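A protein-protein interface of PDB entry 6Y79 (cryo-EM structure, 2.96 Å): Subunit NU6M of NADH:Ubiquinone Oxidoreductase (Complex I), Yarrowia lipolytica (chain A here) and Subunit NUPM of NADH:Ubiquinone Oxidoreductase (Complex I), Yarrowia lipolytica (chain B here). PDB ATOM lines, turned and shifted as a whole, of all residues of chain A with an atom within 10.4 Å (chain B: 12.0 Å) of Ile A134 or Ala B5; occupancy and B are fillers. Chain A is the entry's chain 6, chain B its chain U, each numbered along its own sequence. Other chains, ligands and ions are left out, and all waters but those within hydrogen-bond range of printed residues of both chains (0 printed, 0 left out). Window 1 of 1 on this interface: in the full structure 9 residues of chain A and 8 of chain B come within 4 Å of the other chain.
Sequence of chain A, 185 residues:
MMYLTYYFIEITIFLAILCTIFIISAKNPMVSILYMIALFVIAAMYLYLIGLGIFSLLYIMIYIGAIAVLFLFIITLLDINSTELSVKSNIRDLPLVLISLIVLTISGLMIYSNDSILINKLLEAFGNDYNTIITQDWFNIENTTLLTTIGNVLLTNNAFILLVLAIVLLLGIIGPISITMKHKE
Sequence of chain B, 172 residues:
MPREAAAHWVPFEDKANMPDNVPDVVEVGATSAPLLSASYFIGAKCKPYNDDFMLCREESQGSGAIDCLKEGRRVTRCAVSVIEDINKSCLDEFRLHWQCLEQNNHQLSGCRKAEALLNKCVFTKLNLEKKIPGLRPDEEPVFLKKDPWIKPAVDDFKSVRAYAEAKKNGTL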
ATOM      1  N   TYR A  48       8.101 -27.207  11.711  1.00  0.00           N
ATOM      2  CA  TYR A  48       8.636 -25.889  12.042  1.00  0.00           C
ATOM      3  C   TYR A  48       9.021 -25.815  13.512  1.00  0.00           C
ATOM      4  O   TYR A  48      10.007 -25.165  13.874  1.00  0.00           O
ATOM      5  CB  TYR A  48       7.636 -24.784  11.716  1.00  0.00           C
ATOM      6  CG  TYR A  48       8.196 -23.426  12.066  1.00  0.00           C
ATOM      7  CD1 TYR A  48       9.220 -22.875  11.314  1.00  0.00           C
ATOM      8  CD2 TYR A  48       7.743 -22.719  13.178  1.00  0.00           C
ATOM      9  CE1 TYR A  48       9.760 -21.655  11.633  1.00  0.00           C
ATOM     10  CE2 TYR A  48       8.287 -21.498  13.510  1.00  0.00           C
ATOM     11  CZ  TYR A  48       9.290 -20.970  12.730  1.00  0.00           C
ATOM     12  OH  TYR A  48       9.831 -19.749  13.049  1.00  0.00           O
ATOM     13  N   LEU A  49       8.242 -26.479  14.365  1.00  0.00           N
ATOM     14  CA  LEU A  49       8.458 -26.465  15.803  1.00  0.00           C
ATOM     15  C   LEU A  49       9.796 -27.083  16.179  1.00  0.00           C
ATOM     16  O   LEU A  49      10.517 -26.545  17.020  1.00  0.00           O
ATOM     17  CB  LEU A  49       7.305 -27.216  16.458  1.00  0.00           C
ATOM     18  CG  LEU A  49       6.929 -27.066  17.914  1.00  0.00           C
ATOM     19  CD1 LEU A  49       6.885 -25.608  18.269  1.00  0.00           C
ATOM     20  CD2 LEU A  49       5.565 -27.692  18.078  1.00  0.00           C
ATOM     21  N   ILE A  50      10.160 -28.193  15.540  1.00  0.00           N
ATOM     22  CA  ILE A  50      11.409 -28.870  15.870  1.00  0.00           C
ATOM     23  C   ILE A  50      12.625 -28.145  15.292  1.00  0.00           C
ATOM     24  O   ILE A  50      13.733 -28.279  15.823  1.00  0.00           O
ATOM     25  CB  ILE A  50      11.300 -30.338  15.415  1.00  0.00           C
ATOM     26  CG1 ILE A  50      12.433 -31.186  15.966  1.00  0.00           C
ATOM     27  CG2 ILE A  50      11.266 -30.463  13.915  1.00  0.00           C
ATOM     28  CD1 ILE A  50      12.227 -32.631  15.758  1.00  0.00           C
ATOM     29  N   GLY A  51      12.450 -27.338  14.251  1.00  0.00           N
ATOM     30  CA  GLY A  51      13.553 -26.561  13.724  1.00  0.00           C
ATOM     31  C   GLY A  51      13.706 -26.658  12.223  1.00  0.00           C
ATOM     32  O   GLY A  51      14.611 -26.056  11.645  1.00  0.00           O
ATOM     33  N   LEU A  52      12.833 -27.432  11.588  1.00  0.00           N
ATOM     34  CA  LEU A  52      12.886 -27.676  10.148  1.00  0.00           C
ATOM     35  C   LEU A  52      11.823 -26.838   9.448  1.00  0.00           C
ATOM     36  O   LEU A  52      10.765 -27.325   9.061  1.00  0.00           O
ATOM     37  CB  LEU A  52      12.694 -29.154   9.867  1.00  0.00           C
ATOM     38  CG  LEU A  52      13.759 -30.067  10.451  1.00  0.00           C
ATOM     39  CD1 LEU A  52      13.386 -31.505  10.245  1.00  0.00           C
ATOM     40  CD2 LEU A  52      15.097 -29.775   9.817  1.00  0.00           C
ATOM     41  N   TYR A 130      15.884 -34.245  30.210  1.00  0.00           N
ATOM     42  CA  TYR A 130      17.085 -33.440  30.338  1.00  0.00           C
ATOM     43  C   TYR A 130      17.213 -32.489  29.159  1.00  0.00           C
ATOM     44  O   TYR A 130      16.985 -32.873  28.010  1.00  0.00           O
ATOM     45  CB  TYR A 130      18.285 -34.363  30.506  1.00  0.00           C
ATOM     46  CG  TYR A 130      18.124 -35.057  31.828  1.00  0.00           C
ATOM     47  CD1 TYR A 130      18.391 -34.382  33.004  1.00  0.00           C
ATOM     48  CD2 TYR A 130      17.609 -36.346  31.907  1.00  0.00           C
ATOM     49  CE1 TYR A 130      18.206 -34.979  34.216  1.00  0.00           C
ATOM     50  CE2 TYR A 130      17.416 -36.951  33.117  1.00  0.00           C
ATOM     51  CZ  TYR A 130      17.716 -36.260  34.268  1.00  0.00           C
ATOM     52  OH  TYR A 130      17.518 -36.853  35.480  1.00  0.00           O
ATOM     53  N   ASN A 131      17.537 -31.235  29.462  1.00  0.00           N
ATOM     54  CA  ASN A 131      17.442 -30.141  28.504  1.00  0.00           C
ATOM     55  C   ASN A 131      18.780 -29.985  27.800  1.00  0.00           C
ATOM     56  O   ASN A 131      19.783 -29.678  28.447  1.00  0.00           O
ATOM     57  CB  ASN A 131      17.050 -28.847  29.211  1.00  0.00           C
ATOM     58  CG  ASN A 131      15.564 -28.658  29.289  1.00  0.00           C
ATOM     59  OD1 ASN A 131      14.801 -29.597  29.102  1.00  0.00           O
ATOM     60  ND2 ASN A 131      15.139 -27.431  29.547  1.00  0.00           N
ATOM     61  N   THR A 132      18.792 -30.179  26.481  1.00  0.00           N
ATOM     62  CA  THR A 132      20.037 -30.153  25.721  1.00  0.00           C
ATOM     63  C   THR A 132      20.668 -28.765  25.745  1.00  0.00           C
ATOM     64  O   THR A 132      19.978 -27.747  25.706  1.00  0.00           O
ATOM     65  CB  THR A 132      19.798 -30.649  24.279  1.00  0.00           C
ATOM     66  OG1 THR A 132      21.033 -30.666  23.552  1.00  0.00           O
ATOM     67  CG2 THR A 132      18.761 -29.834  23.531  1.00  0.00           C
ATOM     68  N   ILE A 133      21.982 -28.731  25.916  1.00  0.00           N
ATOM     69  CA  ILE A 133      22.726 -27.480  25.978  1.00  0.00           C
ATOM     70  C   ILE A 133      23.206 -27.148  24.575  1.00  0.00           C
ATOM     71  O   ILE A 133      23.923 -27.940  23.954  1.00  0.00           O
ATOM     72  CB  ILE A 133      23.904 -27.576  26.957  1.00  0.00           C
ATOM     73  CG1 ILE A 133      23.397 -27.695  28.390  1.00  0.00           C
ATOM     74  CG2 ILE A 133      24.809 -26.377  26.813  1.00  0.00           C
ATOM     75  CD1 ILE A 133      24.493 -27.783  29.421  1.00  0.00           C
ATOM     76  N   ILE A 134      22.812 -25.985  24.068  1.00  0.00           N
ATOM     77  CA  ILE A 134      23.201 -25.536  22.739  1.00  0.00           C
ATOM     78  C   ILE A 134      24.354 -24.552  22.883  1.00  0.00           C
ATOM     79  O   ILE A 134      24.232 -23.536  23.576  1.00  0.00           O
ATOM     80  CB  ILE A 134      22.021 -24.907  21.986  1.00  0.00           C
ATOM     81  CG1 ILE A 134      20.940 -25.951  21.722  1.00  0.00           C
ATOM     82  CG2 ILE A 134      22.490 -24.321  20.680  1.00  0.00           C
ATOM     83  CD1 ILE A 134      21.415 -27.111  20.886  1.00  0.00           C
ATOM     84  N   THR A 135      25.467 -24.862  22.228  1.00  0.00           N
ATOM     85  CA  THR A 135      26.700 -24.092  22.261  1.00  0.00           C
ATOM     86  C   THR A 135      26.867 -23.400  20.913  1.00  0.00           C
ATOM     87  O   THR A 135      26.394 -23.898  19.889  1.00  0.00           O
ATOM     88  CB  THR A 135      27.876 -25.043  22.588  1.00  0.00           C
ATOM     89  OG1 THR A 135      27.797 -25.437  23.963  1.00  0.00           O
ATOM     90  CG2 THR A 135      29.282 -24.464  22.328  1.00  0.00           C
ATOM     91  N   GLN A 136      27.488 -22.223  20.909  1.00  0.00           N
ATOM     92  CA  GLN A 136      27.867 -21.576  19.663  1.00  0.00           C
ATOM     93  C   GLN A 136      29.320 -21.853  19.342  1.00  0.00           C
ATOM     94  O   GLN A 136      30.204 -21.632  20.173  1.00  0.00           O
ATOM     95  CB  GLN A 136      27.663 -20.083  19.755  1.00  0.00           C
ATOM     96  CG  GLN A 136      26.285 -19.793  20.076  1.00  0.00           C
ATOM     97  CD  GLN A 136      26.149 -18.369  20.456  1.00  0.00           C
ATOM     98  OE1 GLN A 136      27.092 -17.595  20.352  1.00  0.00           O
ATOM     99  NE2 GLN A 136      25.021 -18.026  21.051  1.00  0.00           N
ATOM    100  N   ASP A 137      29.563 -22.333  18.141  1.00  0.00           N
ATOM    101  CA  ASP A 137      30.902 -22.396  17.593  1.00  0.00           C
ATOM    102  C   ASP A 137      30.916 -21.625  16.285  1.00  0.00           C
ATOM    103  O   ASP A 137      29.951 -21.675  15.518  1.00  0.00           O
ATOM    104  CB  ASP A 137      31.335 -23.843  17.401  1.00  0.00           C
ATOM    105  CG  ASP A 137      30.388 -24.610  16.528  1.00  0.00           C
ATOM    106  OD1 ASP A 137      29.222 -24.791  16.936  1.00  0.00           O
ATOM    107  OD2 ASP A 137      30.801 -25.033  15.434  1.00  0.00           O
ATOM    108  N   PRO B   2      26.461 -25.898  16.645  1.00  0.00           N
ATOM    109  CA  PRO B   2      26.516 -26.192  15.210  1.00  0.00           C
ATOM    110  C   PRO B   2      25.120 -26.221  14.611  1.00  0.00           C
ATOM    111  O   PRO B   2      24.896 -25.719  13.512  1.00  0.00           O
ATOM    112  CB  PRO B   2      27.166 -27.575  15.152  1.00  0.00           C
ATOM    113  CG  PRO B   2      27.781 -27.782  16.499  1.00  0.00           C
ATOM    114  CD  PRO B   2      26.889 -27.049  17.449  1.00  0.00           C
ATOM    115  N   ARG B   3      24.195 -26.824  15.345  1.00  0.00           N
ATOM    116  CA  ARG B   3      22.773 -26.687  15.099  1.00  0.00           C
ATOM    117  C   ARG B   3      22.246 -25.564  15.981  1.00  0.00           C
ATOM    118  O   ARG B   3      22.832 -25.250  17.021  1.00  0.00           O
ATOM    119  CB  ARG B   3      22.033 -27.991  15.400  1.00  0.00           C
ATOM    120  CG  ARG B   3      22.219 -28.478  16.826  1.00  0.00           C
ATOM    121  CD  ARG B   3      21.393 -29.713  17.090  1.00  0.00           C
ATOM    122  NE  ARG B   3      19.990 -29.485  16.766  1.00  0.00           N
ATOM    123  CZ  ARG B   3      19.058 -29.163  17.654  1.00  0.00           C
ATOM    124  NH1 ARG B   3      19.369 -29.044  18.932  1.00  0.00           N
ATOM    125  NH2 ARG B   3      17.809 -28.968  17.261  1.00  0.00           N
ATOM    126  N   GLU B   4      21.160 -24.938  15.541  1.00  0.00           N
ATOM    127  CA  GLU B   4      20.604 -23.802  16.265  1.00  0.00           C
ATOM    128  C   GLU B   4      19.402 -24.230  17.098  1.00  0.00           C
ATOM    129  O   GLU B   4      18.714 -25.201  16.769  1.00  0.00           O
ATOM    130  CB  GLU B   4      20.249 -22.664  15.287  1.00  0.00           C
ATOM    131  CG  GLU B   4      19.181 -22.955  14.253  1.00  0.00           C
ATOM    132  CD  GLU B   4      17.801 -22.556  14.753  1.00  0.00           C
ATOM    133  OE1 GLU B   4      17.731 -21.679  15.641  1.00  0.00           O
ATOM    134  OE2 GLU B   4      16.822 -23.146  14.278  1.00  0.00           O
ATOM    135  N   ALA B   5      19.176 -23.517  18.202  1.00  0.00           N
ATOM    136  CA  ALA B   5      18.145 -23.909  19.157  1.00  0.00           C
ATOM    137  C   ALA B   5      16.758 -23.510  18.663  1.00  0.00           C
ATOM    138  O   ALA B   5      16.527 -22.367  18.265  1.00  0.00           O
ATOM    139  CB  ALA B   5      18.417 -23.270  20.519  1.00  0.00           C
ATOM    140  N   ALA B   6      15.834 -24.456  18.712  1.00  0.00           N
ATOM    141  CA  ALA B   6      14.441 -24.254  18.374  1.00  0.00           C
ATOM    142  C   ALA B   6      13.627 -24.751  19.559  1.00  0.00           C
ATOM    143  O   ALA B   6      14.170 -25.191  20.556  1.00  0.00           O
ATOM    144  CB  ALA B   6      14.046 -25.012  17.104  1.00  0.00           C
ATOM    145  N   ALA B   7      12.311 -24.606  19.459  1.00  0.00           N
ATOM    146  CA  ALA B   7      11.316 -25.230  20.332  1.00  0.00           C
ATOM    147  C   ALA B   7      11.552 -24.881  21.799  1.00  0.00           C
ATOM    148  O   ALA B   7      11.943 -25.735  22.561  1.00  0.00           O
ATOM    149  CB  ALA B   7      11.297 -26.755  20.142  1.00  0.00           C
ATOM    150  N   HIS B   8      11.414 -23.593  22.116  1.00  0.00           N
ATOM    151  CA  HIS B   8      11.490 -23.078  23.479  1.00  0.00           C
ATOM    152  C   HIS B   8      12.854 -23.364  24.130  1.00  0.00           C
ATOM    153  O   HIS B   8      12.976 -24.116  25.101  1.00  0.00           O
ATOM    154  CB  HIS B   8      10.332 -23.646  24.314  1.00  0.00           C
ATOM    155  CG  HIS B   8      10.188 -23.033  25.673  1.00  0.00           C
ATOM    156  ND1 HIS B   8      10.710 -23.614  26.807  1.00  0.00           N
ATOM    157  CD2 HIS B   8       9.587 -21.890  26.077  1.00  0.00           C
ATOM    158  CE1 HIS B   8      10.431 -22.859  27.853  1.00  0.00           C
ATOM    159  NE2 HIS B   8       9.753 -21.805  27.437  1.00  0.00           N
ATOM    160  N   TRP B   9      13.900 -22.776  23.568  1.00  0.00           N
ATOM    161  CA  TRP B   9      15.148 -22.648  24.303  1.00  0.00           C
ATOM    162  C   TRP B   9      15.011 -21.495  25.292  1.00  0.00           C
ATOM    163  O   TRP B   9      14.405 -20.467  24.987  1.00  0.00           O
ATOM    164  CB  TRP B   9      16.309 -22.385  23.341  1.00  0.00           C
ATOM    165  CG  TRP B   9      16.165 -21.104  22.542  1.00  0.00           C
ATOM    166  CD1 TRP B   9      15.464 -20.926  21.385  1.00  0.00           C
ATOM    167  CD2 TRP B   9      16.719 -19.828  22.873  1.00  0.00           C
ATOM    168  NE1 TRP B   9      15.552 -19.617  20.975  1.00  0.00           N
ATOM    169  CE2 TRP B   9      16.319 -18.923  21.873  1.00  0.00           C
ATOM    170  CE3 TRP B   9      17.512 -19.363  23.919  1.00  0.00           C
ATOM    171  CZ2 TRP B   9      16.692 -17.582  21.890  1.00  0.00           C
ATOM    172  CZ3 TRP B   9      17.889 -18.039  23.927  1.00  0.00           C
ATOM    173  CH2 TRP B   9      17.474 -17.160  22.926  1.00  0.00           C
ATOM    174  N   VAL B  10      15.563 -21.661  26.491  1.00  0.00           N
ATOM    175  CA  VAL B  10      15.642 -20.564  27.449  1.00  0.00           C
ATOM    176  C   VAL B  10      17.096 -20.288  27.797  1.00  0.00           C
ATOM    177  O   VAL B  10      17.877 -21.221  28.016  1.00  0.00           O
ATOM    178  CB  VAL B  10      14.779 -20.759  28.716  1.00  0.00           C
ATOM    179  CG1 VAL B  10      13.314 -20.905  28.319  1.00  0.00           C
ATOM    180  CG2 VAL B  10      15.227 -21.934  29.635  1.00  0.00           C
ATOM    181  N   PRO B  11      17.529 -19.029  27.772  1.00  0.00           N
ATOM    182  CA  PRO B  11      18.950 -18.722  27.949  1.00  0.00           C
ATOM    183  C   PRO B  11      19.356 -18.695  29.411  1.00  0.00           C
ATOM    184  O   PRO B  11      18.566 -18.366  30.298  1.00  0.00           O
ATOM    185  CB  PRO B  11      19.097 -17.341  27.301  1.00  0.00           C
ATOM    186  CG  PRO B  11      17.747 -16.760  27.310  1.00  0.00           C
ATOM    187  CD  PRO B  11      16.751 -17.860  27.322  1.00  0.00           C
ATOM    188  N   PHE B  12      20.606 -19.057  29.660  1.00  0.00           N
ATOM    189  CA  PHE B  12      21.089 -19.107  31.028  1.00  0.00           C
ATOM    190  C   PHE B  12      22.563 -18.756  31.075  1.00  0.00           C
ATOM    191  O   PHE B  12      23.323 -19.084  30.160  1.00  0.00           O
ATOM    192  CB  PHE B  12      20.843 -20.480  31.687  1.00  0.00           C
ATOM    193  CG  PHE B  12      21.656 -21.595  31.115  1.00  0.00           C
ATOM    194  CD1 PHE B  12      21.272 -22.210  29.942  1.00  0.00           C
ATOM    195  CD2 PHE B  12      22.787 -22.054  31.768  1.00  0.00           C
ATOM    196  CE1 PHE B  12      22.012 -23.237  29.415  1.00  0.00           C
ATOM    197  CE2 PHE B  12      23.531 -23.088  31.241  1.00  0.00           C
ATOM    198  CZ  PHE B  12      23.147 -23.671  30.064  1.00  0.00           C
ATOM    199  N   GLU B  13      22.959 -18.087  32.147  1.00  0.00           N
ATOM    200  CA  GLU B  13      24.337 -17.673  32.304  1.00  0.00           C
ATOM    201  C   GLU B  13      24.879 -18.095  33.654  1.00  0.00           C
ATOM    202  O   GLU B  13      24.155 -18.597  34.511  1.00  0.00           O
ATOM    203  CB  GLU B  13      24.490 -16.173  32.120  1.00  0.00           C
ATOM    204  CG  GLU B  13      23.936 -15.320  33.164  1.00  0.00           C
ATOM    205  CD  GLU B  13      22.494 -14.892  32.919  1.00  0.00           C
ATOM    206  OE1 GLU B  13      21.740 -15.578  32.209  1.00  0.00           O
ATOM    207  OE2 GLU B  13      22.193 -13.767  33.338  1.00  0.00           O
ATOM    208  N   ASP B  14      26.170 -17.847  33.840  1.00  0.00           N
ATOM    209  CA  ASP B  14      26.931 -18.567  34.847  1.00  0.00           C
ATOM    210  C   ASP B  14      27.750 -17.604  35.693  1.00  0.00           C
ATOM    211  O   ASP B  14      28.672 -16.944  35.194  1.00  0.00           O
ATOM    212  CB  ASP B  14      27.815 -19.609  34.179  1.00  0.00           C
ATOM    213  CG  ASP B  14      28.637 -20.368  35.166  1.00  0.00           C
ATOM    214  OD1 ASP B  14      28.078 -21.170  35.944  1.00  0.00           O
ATOM    215  OD2 ASP B  14      29.861 -20.183  35.132  1.00  0.00           O
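The side-chain carboxylate (OD1) of Asp A137 lies close to the backbone nitrogen (N) of Pro B2 (3.0 Å).
Among the printed residues, merely in contact across the chains: Leu A49 with Ala B7 (3.2 Å), Ile A134 with Arg B3 (3.4 Å), Ile A50 with Ala B6 (3.5 Å), Gly A51 with Ala B6 (3.8 Å), Thr A135 with Pro B2 (3.8 Å), Leu A49 with Ala B6 (3.8 Å) and Ile A134 with Ala B5 (3.9 Å).
Of the printed residues of chain B, Leu A49 touches Ala B6 and Ala B7. Of the printed residues of chain B, Ile A50 touches Ala B6 (3.5 Å). Printed residues of chain B within 4 Å of Gly A51: Ala B6 (3.8 Å). Tyr A130 touches none of the printed residues of chain B. Ile A133 touches none of the printed residues of chain B. Of chain B, only Arg B3 and Ala B5 come within 4 Å of Ile A134. Thr A135 touches just one residue of chain B: Pro B2 (3.8 Å). No residue of chain B comes within 4 Å of Gln A136. Of the printed residues of chain B, Asp A137 touches Pro B2 (3.0 Å). Printed residues of chain A within 4 Å of Pro B2: Thr A135 (3.8 Å) and Asp A137 (3.0 Å). Arg B3 touches just one residue of chain A: Ile A134 (3.4 Å). No residue of chain A comes within 4 Å of Glu B4. Ala B5 touches one residue of chain A. Printed residues of chain A within 4 Å of Ala B7: Leu A49 (3.2 Å). The nearest residue of chain B that does not touch Ile A134 is Glu B4 (4.7 Å). The nearest residue of chain A that does not touch Ala B5 is Ile A50 (6.3 Å).
Hydrophobic or aromatic side chains of chain A that line the printed part of chain B: Ile A134. Among the printed residues, 8 pairs touch across the chains.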
